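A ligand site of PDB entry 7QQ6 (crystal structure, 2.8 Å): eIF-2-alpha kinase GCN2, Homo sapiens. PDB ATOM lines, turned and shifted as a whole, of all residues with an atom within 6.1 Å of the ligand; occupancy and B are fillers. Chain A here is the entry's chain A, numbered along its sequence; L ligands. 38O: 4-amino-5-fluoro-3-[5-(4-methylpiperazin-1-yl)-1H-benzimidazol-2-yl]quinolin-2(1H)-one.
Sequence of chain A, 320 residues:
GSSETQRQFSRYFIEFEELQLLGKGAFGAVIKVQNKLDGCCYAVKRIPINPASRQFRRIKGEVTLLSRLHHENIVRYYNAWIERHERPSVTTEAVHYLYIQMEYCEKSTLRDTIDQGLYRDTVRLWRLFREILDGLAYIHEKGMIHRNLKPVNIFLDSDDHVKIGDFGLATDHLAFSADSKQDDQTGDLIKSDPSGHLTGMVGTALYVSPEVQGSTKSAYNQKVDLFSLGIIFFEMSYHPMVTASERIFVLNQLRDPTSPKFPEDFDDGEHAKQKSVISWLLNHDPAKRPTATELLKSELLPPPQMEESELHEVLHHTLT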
ATOM      1  N   GLN A  20      30.618  12.293 -20.795  1.00  0.00           N
ATOM      2  CA  GLN A  20      29.305  12.440 -20.164  1.00  0.00           C
ATOM      3  C   GLN A  20      28.520  11.134 -20.259  1.00  0.00           C
ATOM      4  O   GLN A  20      28.557  10.503 -21.293  1.00  0.00           O
ATOM      5  CB  GLN A  20      28.521  13.528 -20.914  1.00  0.00           C
ATOM      6  CG  GLN A  20      27.336  14.089 -20.170  1.00  0.00           C
ATOM      7  CD  GLN A  20      26.493  14.884 -21.107  1.00  0.00           C
ATOM      8  OE1 GLN A  20      26.761  16.060 -21.346  1.00  0.00           O
ATOM      9  NE2 GLN A  20      25.475  14.254 -21.668  1.00  0.00           N
ATOM     10  N   LEU A  22      25.214   9.194 -21.069  1.00  0.00           N
ATOM     11  CA  LEU A  22      24.010   9.504 -21.879  1.00  0.00           C
ATOM     12  C   LEU A  22      22.753   8.732 -21.406  1.00  0.00           C
ATOM     13  O   LEU A  22      21.648   9.299 -21.442  1.00  0.00           O
ATOM     14  CB  LEU A  22      24.252   9.323 -23.401  1.00  0.00           C
ATOM     15  CG  LEU A  22      25.310  10.220 -24.074  1.00  0.00           C
ATOM     16  CD1 LEU A  22      25.544   9.811 -25.520  1.00  0.00           C
ATOM     17  CD2 LEU A  22      24.925  11.692 -24.005  1.00  0.00           C
ATOM     18  N   GLY A  23      22.945   7.500 -20.936  1.00  0.00           N
ATOM     19  CA  GLY A  23      21.917   6.607 -20.410  1.00  0.00           C
ATOM     20  C   GLY A  23      22.480   5.494 -19.556  1.00  0.00           C
ATOM     21  O   GLY A  23      23.672   5.201 -19.607  1.00  0.00           O
ATOM     22  N   VAL A  30      25.278   3.888 -21.806  1.00  0.00           N
ATOM     23  CA  VAL A  30      25.616   4.581 -23.059  1.00  0.00           C
ATOM     24  C   VAL A  30      26.419   5.803 -22.574  1.00  0.00           C
ATOM     25  O   VAL A  30      25.972   6.489 -21.663  1.00  0.00           O
ATOM     26  CB  VAL A  30      24.355   4.968 -23.902  1.00  0.00           C
ATOM     27  CG1 VAL A  30      24.738   5.767 -25.153  1.00  0.00           C
ATOM     28  CG2 VAL A  30      23.539   3.744 -24.293  1.00  0.00           C
ATOM     29  N   ALA A  43      28.695   7.686 -29.180  1.00  0.00           N
ATOM     30  CA  ALA A  43      27.860   7.143 -28.134  1.00  0.00           C
ATOM     31  C   ALA A  43      28.198   5.660 -28.108  1.00  0.00           C
ATOM     32  O   ALA A  43      27.716   4.906 -28.947  1.00  0.00           O
ATOM     33  CB  ALA A  43      26.401   7.393 -28.424  1.00  0.00           C
ATOM     34  N   LYS A  45      28.069   2.100 -26.368  1.00  0.00           N
ATOM     35  CA  LYS A  45      27.144   1.320 -25.537  1.00  0.00           C
ATOM     36  C   LYS A  45      27.953   0.173 -24.967  1.00  0.00           C
ATOM     37  O   LYS A  45      28.431  -0.661 -25.740  1.00  0.00           O
ATOM     38  CB  LYS A  45      25.963   0.785 -26.402  1.00  0.00           C
ATOM     39  CG  LYS A  45      24.713   0.358 -25.623  1.00  0.00           C
ATOM     40  CD  LYS A  45      23.700  -0.384 -26.505  1.00  0.00           C
ATOM     41  CE  LYS A  45      22.287  -0.423 -25.959  1.00  0.00           C
ATOM     42  NZ  LYS A  45      21.315   0.324 -26.835  1.00  0.00           N
ATOM     43  N   VAL A  75      20.788   5.508 -36.885  1.00  0.00           N
ATOM     44  CA  VAL A  75      21.987   5.942 -36.167  1.00  0.00           C
ATOM     45  C   VAL A  75      23.160   5.114 -36.741  1.00  0.00           C
ATOM     46  O   VAL A  75      23.021   3.897 -36.954  1.00  0.00           O
ATOM     47  CB  VAL A  75      21.758   5.836 -34.634  1.00  0.00           C
ATOM     48  CG1 VAL A  75      22.291   4.533 -34.028  1.00  0.00           C
ATOM     49  CG2 VAL A  75      22.281   7.067 -33.921  1.00  0.00           C
ATOM     50  N   MET A 102      28.764   4.000 -31.732  1.00  0.00           N
ATOM     51  CA  MET A 102      27.773   4.531 -32.660  1.00  0.00           C
ATOM     52  C   MET A 102      27.829   6.035 -32.742  1.00  0.00           C
ATOM     53  O   MET A 102      28.576   6.634 -31.963  1.00  0.00           O
ATOM     54  CB  MET A 102      26.360   4.021 -32.311  1.00  0.00           C
ATOM     55  CG  MET A 102      26.189   2.548 -32.576  1.00  0.00           C
ATOM     56  SD  MET A 102      24.731   1.868 -31.793  1.00  0.00           S
ATOM     57  CE  MET A 102      25.152   2.136 -30.022  1.00  0.00           C
ATOM     58  N   GLU A 103      27.080   6.669 -33.661  1.00  0.00           N
ATOM     59  CA  GLU A 103      27.192   8.121 -33.819  1.00  0.00           C
ATOM     60  C   GLU A 103      26.582   8.885 -32.676  1.00  0.00           C
ATOM     61  O   GLU A 103      25.672   8.382 -32.019  1.00  0.00           O
ATOM     62  CB  GLU A 103      26.674   8.636 -35.185  1.00  0.00           C
ATOM     63  CG  GLU A 103      25.170   8.762 -35.346  1.00  0.00           C
ATOM     64  CD  GLU A 103      24.729   9.504 -36.588  1.00  0.00           C
ATOM     65  OE1 GLU A 103      24.877  10.742 -36.641  1.00  0.00           O
ATOM     66  OE2 GLU A 103      24.221   8.833 -37.515  1.00  0.00           O
ATOM     67  N   TYR A 104      27.140  10.076 -32.420  1.00  0.00           N
ATOM     68  CA  TYR A 104      26.658  10.988 -31.410  1.00  0.00           C
ATOM     69  C   TYR A 104      25.876  12.059 -32.144  1.00  0.00           C
ATOM     70  O   TYR A 104      26.435  12.777 -32.990  1.00  0.00           O
ATOM     71  CB  TYR A 104      27.800  11.545 -30.521  1.00  0.00           C
ATOM     72  CG  TYR A 104      27.319  12.607 -29.565  1.00  0.00           C
ATOM     73  CD1 TYR A 104      26.505  12.274 -28.486  1.00  0.00           C
ATOM     74  CD2 TYR A 104      27.605  13.949 -29.779  1.00  0.00           C
ATOM     75  CE1 TYR A 104      25.966  13.264 -27.667  1.00  0.00           C
ATOM     76  CE2 TYR A 104      27.068  14.947 -28.963  1.00  0.00           C
ATOM     77  CZ  TYR A 104      26.261  14.597 -27.899  1.00  0.00           C
ATOM     78  OH  TYR A 104      25.747  15.569 -27.074  1.00  0.00           O
ATOM     79  N   CYS A 105      24.562  12.073 -31.912  1.00  0.00           N
ATOM     80  CA  CYS A 105      23.611  13.001 -32.507  1.00  0.00           C
ATOM     81  C   CYS A 105      23.560  14.185 -31.551  1.00  0.00           C
ATOM     82  O   CYS A 105      22.995  14.106 -30.464  1.00  0.00           O
ATOM     83  CB  CYS A 105      22.247  12.350 -32.719  1.00  0.00           C
ATOM     84  SG  CYS A 105      22.263  10.988 -33.927  1.00  0.00           S
ATOM     85  N   GLU A 106      24.279  15.227 -31.933  1.00  0.00           N
ATOM     86  CA  GLU A 106      24.523  16.456 -31.188  1.00  0.00           C
ATOM     87  C   GLU A 106      23.281  17.195 -30.706  1.00  0.00           C
ATOM     88  O   GLU A 106      23.263  17.660 -29.571  1.00  0.00           O
ATOM     89  CB  GLU A 106      25.381  17.425 -32.014  1.00  0.00           C
ATOM     90  CG  GLU A 106      26.395  16.784 -32.949  1.00  0.00           C
ATOM     91  CD  GLU A 106      27.734  17.514 -32.917  1.00  0.00           C
ATOM     92  OE1 GLU A 106      27.831  18.603 -33.532  1.00  0.00           O
ATOM     93  OE2 GLU A 106      28.662  17.007 -32.258  1.00  0.00           O
ATOM     94  N   LYS A 107      22.279  17.348 -31.588  1.00  0.00           N
ATOM     95  CA  LYS A 107      21.064  18.133 -31.379  1.00  0.00           C
ATOM     96  C   LYS A 107      19.964  17.411 -30.602  1.00  0.00           C
ATOM     97  O   LYS A 107      18.825  17.400 -31.066  1.00  0.00           O
ATOM     98  CB  LYS A 107      20.540  18.630 -32.740  1.00  0.00           C
ATOM     99  CG  LYS A 107      20.150  20.093 -32.825  1.00  0.00           C
ATOM    100  CD  LYS A 107      18.666  20.321 -32.557  1.00  0.00           C
ATOM    101  CE  LYS A 107      17.853  20.492 -33.801  1.00  0.00           C
ATOM    102  NZ  LYS A 107      18.082  21.799 -34.487  1.00  0.00           N
ATOM    103  N   SER A 108      20.290  16.809 -29.436  1.00  0.00           N
ATOM    104  CA  SER A 108      19.355  16.142 -28.493  1.00  0.00           C
ATOM    105  C   SER A 108      18.641  14.858 -29.009  1.00  0.00           C
ATOM    106  O   SER A 108      18.911  14.366 -30.117  1.00  0.00           O
ATOM    107  CB  SER A 108      18.304  17.153 -28.011  1.00  0.00           C
ATOM    108  OG  SER A 108      17.266  17.434 -28.951  1.00  0.00           O
ATOM    109  N   THR A 109      17.712  14.338 -28.160  1.00  0.00           N
ATOM    110  CA  THR A 109      16.825  13.210 -28.415  1.00  0.00           C
ATOM    111  C   THR A 109      15.476  13.790 -28.912  1.00  0.00           C
ATOM    112  O   THR A 109      15.255  14.996 -28.801  1.00  0.00           O
ATOM    113  CB  THR A 109      16.551  12.442 -27.107  1.00  0.00           C
ATOM    114  OG1 THR A 109      16.005  13.357 -26.173  1.00  0.00           O
ATOM    115  CG2 THR A 109      17.798  11.817 -26.507  1.00  0.00           C
ATOM    116  N   ASP A 112      13.429  15.236 -25.735  1.00  0.00           N
ATOM    117  CA  ASP A 112      13.711  16.630 -25.371  1.00  0.00           C
ATOM    118  C   ASP A 112      13.215  17.645 -26.412  1.00  0.00           C
ATOM    119  O   ASP A 112      12.969  18.807 -26.061  1.00  0.00           O
ATOM    120  CB  ASP A 112      15.205  16.773 -25.048  1.00  0.00           C
ATOM    121  CG  ASP A 112      15.586  15.973 -23.812  1.00  0.00           C
ATOM    122  OD1 ASP A 112      15.805  14.755 -23.929  1.00  0.00           O
ATOM    123  OD2 ASP A 112      15.589  16.551 -22.719  1.00  0.00           O
ATOM    124  N   VAL A 152      13.172   8.408 -26.436  1.00  0.00           N
ATOM    125  CA  VAL A 152      14.506   8.453 -25.840  1.00  0.00           C
ATOM    126  C   VAL A 152      15.533   7.688 -26.687  1.00  0.00           C
ATOM    127  O   VAL A 152      16.742   7.834 -26.437  1.00  0.00           O
ATOM    128  CB  VAL A 152      14.542   8.029 -24.361  1.00  0.00           C
ATOM    129  CG1 VAL A 152      13.952   9.123 -23.470  1.00  0.00           C
ATOM    130  CG2 VAL A 152      13.836   6.695 -24.143  1.00  0.00           C
ATOM    131  N   ASN A 153      15.060   6.923 -27.710  1.00  0.00           N
ATOM    132  CA  ASN A 153      15.844   6.119 -28.658  1.00  0.00           C
ATOM    133  C   ASN A 153      15.682   6.566 -30.169  1.00  0.00           C
ATOM    134  O   ASN A 153      15.838   5.762 -31.086  1.00  0.00           O
ATOM    135  CB  ASN A 153      15.505   4.641 -28.448  1.00  0.00           C
ATOM    136  CG  ASN A 153      16.490   3.675 -29.050  1.00  0.00           C
ATOM    137  OD1 ASN A 153      17.695   3.690 -28.762  1.00  0.00           O
ATOM    138  ND2 ASN A 153      15.957   2.794 -29.895  1.00  0.00           N
ATOM    139  N   PHE A 155      16.852  10.354 -32.210  1.00  0.00           N
ATOM    140  CA  PHE A 155      17.670  11.527 -31.960  1.00  0.00           C
ATOM    141  C   PHE A 155      17.727  12.460 -33.147  1.00  0.00           C
ATOM    142  O   PHE A 155      17.242  12.103 -34.216  1.00  0.00           O
ATOM    143  CB  PHE A 155      19.108  11.108 -31.518  1.00  0.00           C
ATOM    144  CG  PHE A 155      19.211   9.897 -30.620  1.00  0.00           C
ATOM    145  CD1 PHE A 155      18.984   9.997 -29.250  1.00  0.00           C
ATOM    146  CD2 PHE A 155      19.491   8.640 -31.151  1.00  0.00           C
ATOM    147  CE1 PHE A 155      19.019   8.874 -28.433  1.00  0.00           C
ATOM    148  CE2 PHE A 155      19.558   7.518 -30.333  1.00  0.00           C
ATOM    149  CZ  PHE A 155      19.296   7.639 -28.970  1.00  0.00           C
ATOM    150  N   GLY A 165      17.565   5.240 -33.167  1.00  0.00           N
ATOM    151  CA  GLY A 165      18.593   4.576 -32.355  1.00  0.00           C
ATOM    152  C   GLY A 165      18.700   3.083 -32.615  1.00  0.00           C
ATOM    153  O   GLY A 165      17.963   2.538 -33.420  1.00  0.00           O
ATOM    154  N   ASP A 166      19.618   2.427 -31.913  1.00  0.00           N
ATOM    155  CA  ASP A 166      19.800   0.984 -32.060  1.00  0.00           C
ATOM    156  C   ASP A 166      18.722   0.199 -31.285  1.00  0.00           C
ATOM    157  O   ASP A 166      17.846   0.807 -30.690  1.00  0.00           O
ATOM    158  CB  ASP A 166      21.221   0.594 -31.574  1.00  0.00           C
ATOM    159  CG  ASP A 166      21.458   0.708 -30.078  1.00  0.00           C
ATOM    160  OD1 ASP A 166      21.176   1.782 -29.494  1.00  0.00           O
ATOM    161  OD2 ASP A 166      21.956  -0.279 -29.482  1.00  0.00           O
HETATM  162  C1  38O L   1      17.953  16.697 -20.492  1.00  0.00           C
HETATM  163  C3  38O L   1      19.348  16.843 -22.445  1.00  0.00           C
HETATM  164  C4  38O L   1      19.739  16.184 -23.761  1.00  0.00           C
HETATM  165  C6  38O L   1      19.264  14.027 -22.775  1.00  0.00           C
HETATM  166  C7  38O L   1      18.887  14.717 -21.488  1.00  0.00           C
HETATM  167  C8  38O L   1      20.894  14.213 -24.565  1.00  0.00           C
HETATM  168  C12 38O L   1      22.326  10.947 -27.379  1.00  0.00           C
HETATM  169  N13 38O L   1      22.798  12.150 -27.661  1.00  0.00           N
HETATM  170  C15 38O L   1      22.389  14.356 -26.483  1.00  0.00           C
HETATM  171  C16 38O L   1      21.716  14.954 -25.429  1.00  0.00           C
HETATM  172  C17 38O L   1      22.607   9.708 -28.124  1.00  0.00           C
HETATM  173  C18 38O L   1      22.236   8.471 -27.641  1.00  0.00           C
HETATM  174  C21 38O L   1      22.248   5.975 -28.082  1.00  0.00           C
HETATM  175  C23 38O L   1      22.562   4.890 -28.860  1.00  0.00           C
HETATM  176  C24 38O L   1      23.215   5.104 -30.056  1.00  0.00           C
HETATM  177  O29 38O L   1      23.624  10.990 -29.827  1.00  0.00           O
HETATM  178  N2  38O L   1      18.348  16.042 -21.746  1.00  0.00           N
HETATM  179  N5  38O L   1      20.237  14.826 -23.516  1.00  0.00           N
HETATM  180  C9  38O L   1      20.756  12.833 -24.773  1.00  0.00           C
HETATM  181  C10 38O L   1      21.432  12.242 -25.838  1.00  0.00           C
HETATM  182  N11 38O L   1      21.498  10.938 -26.301  1.00  0.00           N
HETATM  183  C14 38O L   1      22.244  12.988 -26.694  1.00  0.00           C
HETATM  184  N19 38O L   1      21.596   8.288 -26.475  1.00  0.00           N
HETATM  185  C20 38O L   1      22.551   7.284 -28.431  1.00  0.00           C
HETATM  186  F22 38O L   1      21.601   5.774 -26.910  1.00  0.00           F
HETATM  187  C25 38O L   1      23.549   6.387 -30.460  1.00  0.00           C
HETATM  188  C26 38O L   1      23.225   7.481 -29.664  1.00  0.00           C
HETATM  189  N27 38O L   1      23.558   8.761 -30.077  1.00  0.00           N
HETATM  190  C28 38O L   1      23.291   9.896 -29.374  1.00  0.00           C
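N of Cys 105 is in hydrogen-bond range of O29 of the ligand (2.5 Å). N13 of the ligand sits at hydrogen-bond distance from O of Cys 105 (3.4 Å). The backbone carbonyl oxygen (O) of Glu 103 lies within hydrogen-bond range of a nitrogen (N27) of the ligand (2.9 Å). A nitrogen (N2) of the ligand is in salt-bridge range of the side-chain carboxylate (OD2) of Asp 112, at 3.0 Å.
The side-chain carboxylate (OE1) of Glu 103 lies within hydrogen-bond range of the side-chain sulfur (SG) of Cys 105 (3.8 Å). OG1 of Thr 109 sits at hydrogen-bond distance from OD1 of Asp 112, 2.7 Å away. N of Ala 43 lies within hydrogen-bond range of O of Met 102, 3.0 Å away. The backbone carbonyl oxygen of Asp 166 is in hydrogen-bond range of the side-chain amide nitrogen of Asn 153, at 2.9 Å. The side-chain amino group (NZ) of Lys 45 lies within salt-bridge range of the side-chain carboxylate (OD2) of Asp 166 (2.8 Å). The backbone NH (N) of Leu 22 is in hydrogen-bond range of the backbone carbonyl oxygen (O) of Val 30 (2.9 Å). The backbone NH (N) of Val 30 lies within hydrogen-bond range of the backbone carbonyl oxygen (O) of Gly 23.
CD1 of Leu 22 touches C12 of the ligand, 3.9 Å away. Val 30 touches the ligand (CG1 to F22, 3.6 Å). Ala 43 touches the ligand (CB to C26, 3.4 Å). CG2 of Val 75 touches C25 of the ligand, at 3.7 Å. CE of Met 102 touches C24 of the ligand, 3.5 Å away. Tyr 104 touches the ligand (CE1 to N13, 3.4 Å). CG2 of Thr 109 touches C9 of the ligand, 3.6 Å away. Phe 155 touches the ligand (CE1 to N19, 3.3 Å). Asp 166 touches the ligand (OD1 to C23, 3.5 Å). Hydrophobic or aromatic side chains within 4 Å of the ligand: Leu 22, Val 30, Ala 43, Val 75, Met 102, Tyr 104 and Phe 155.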
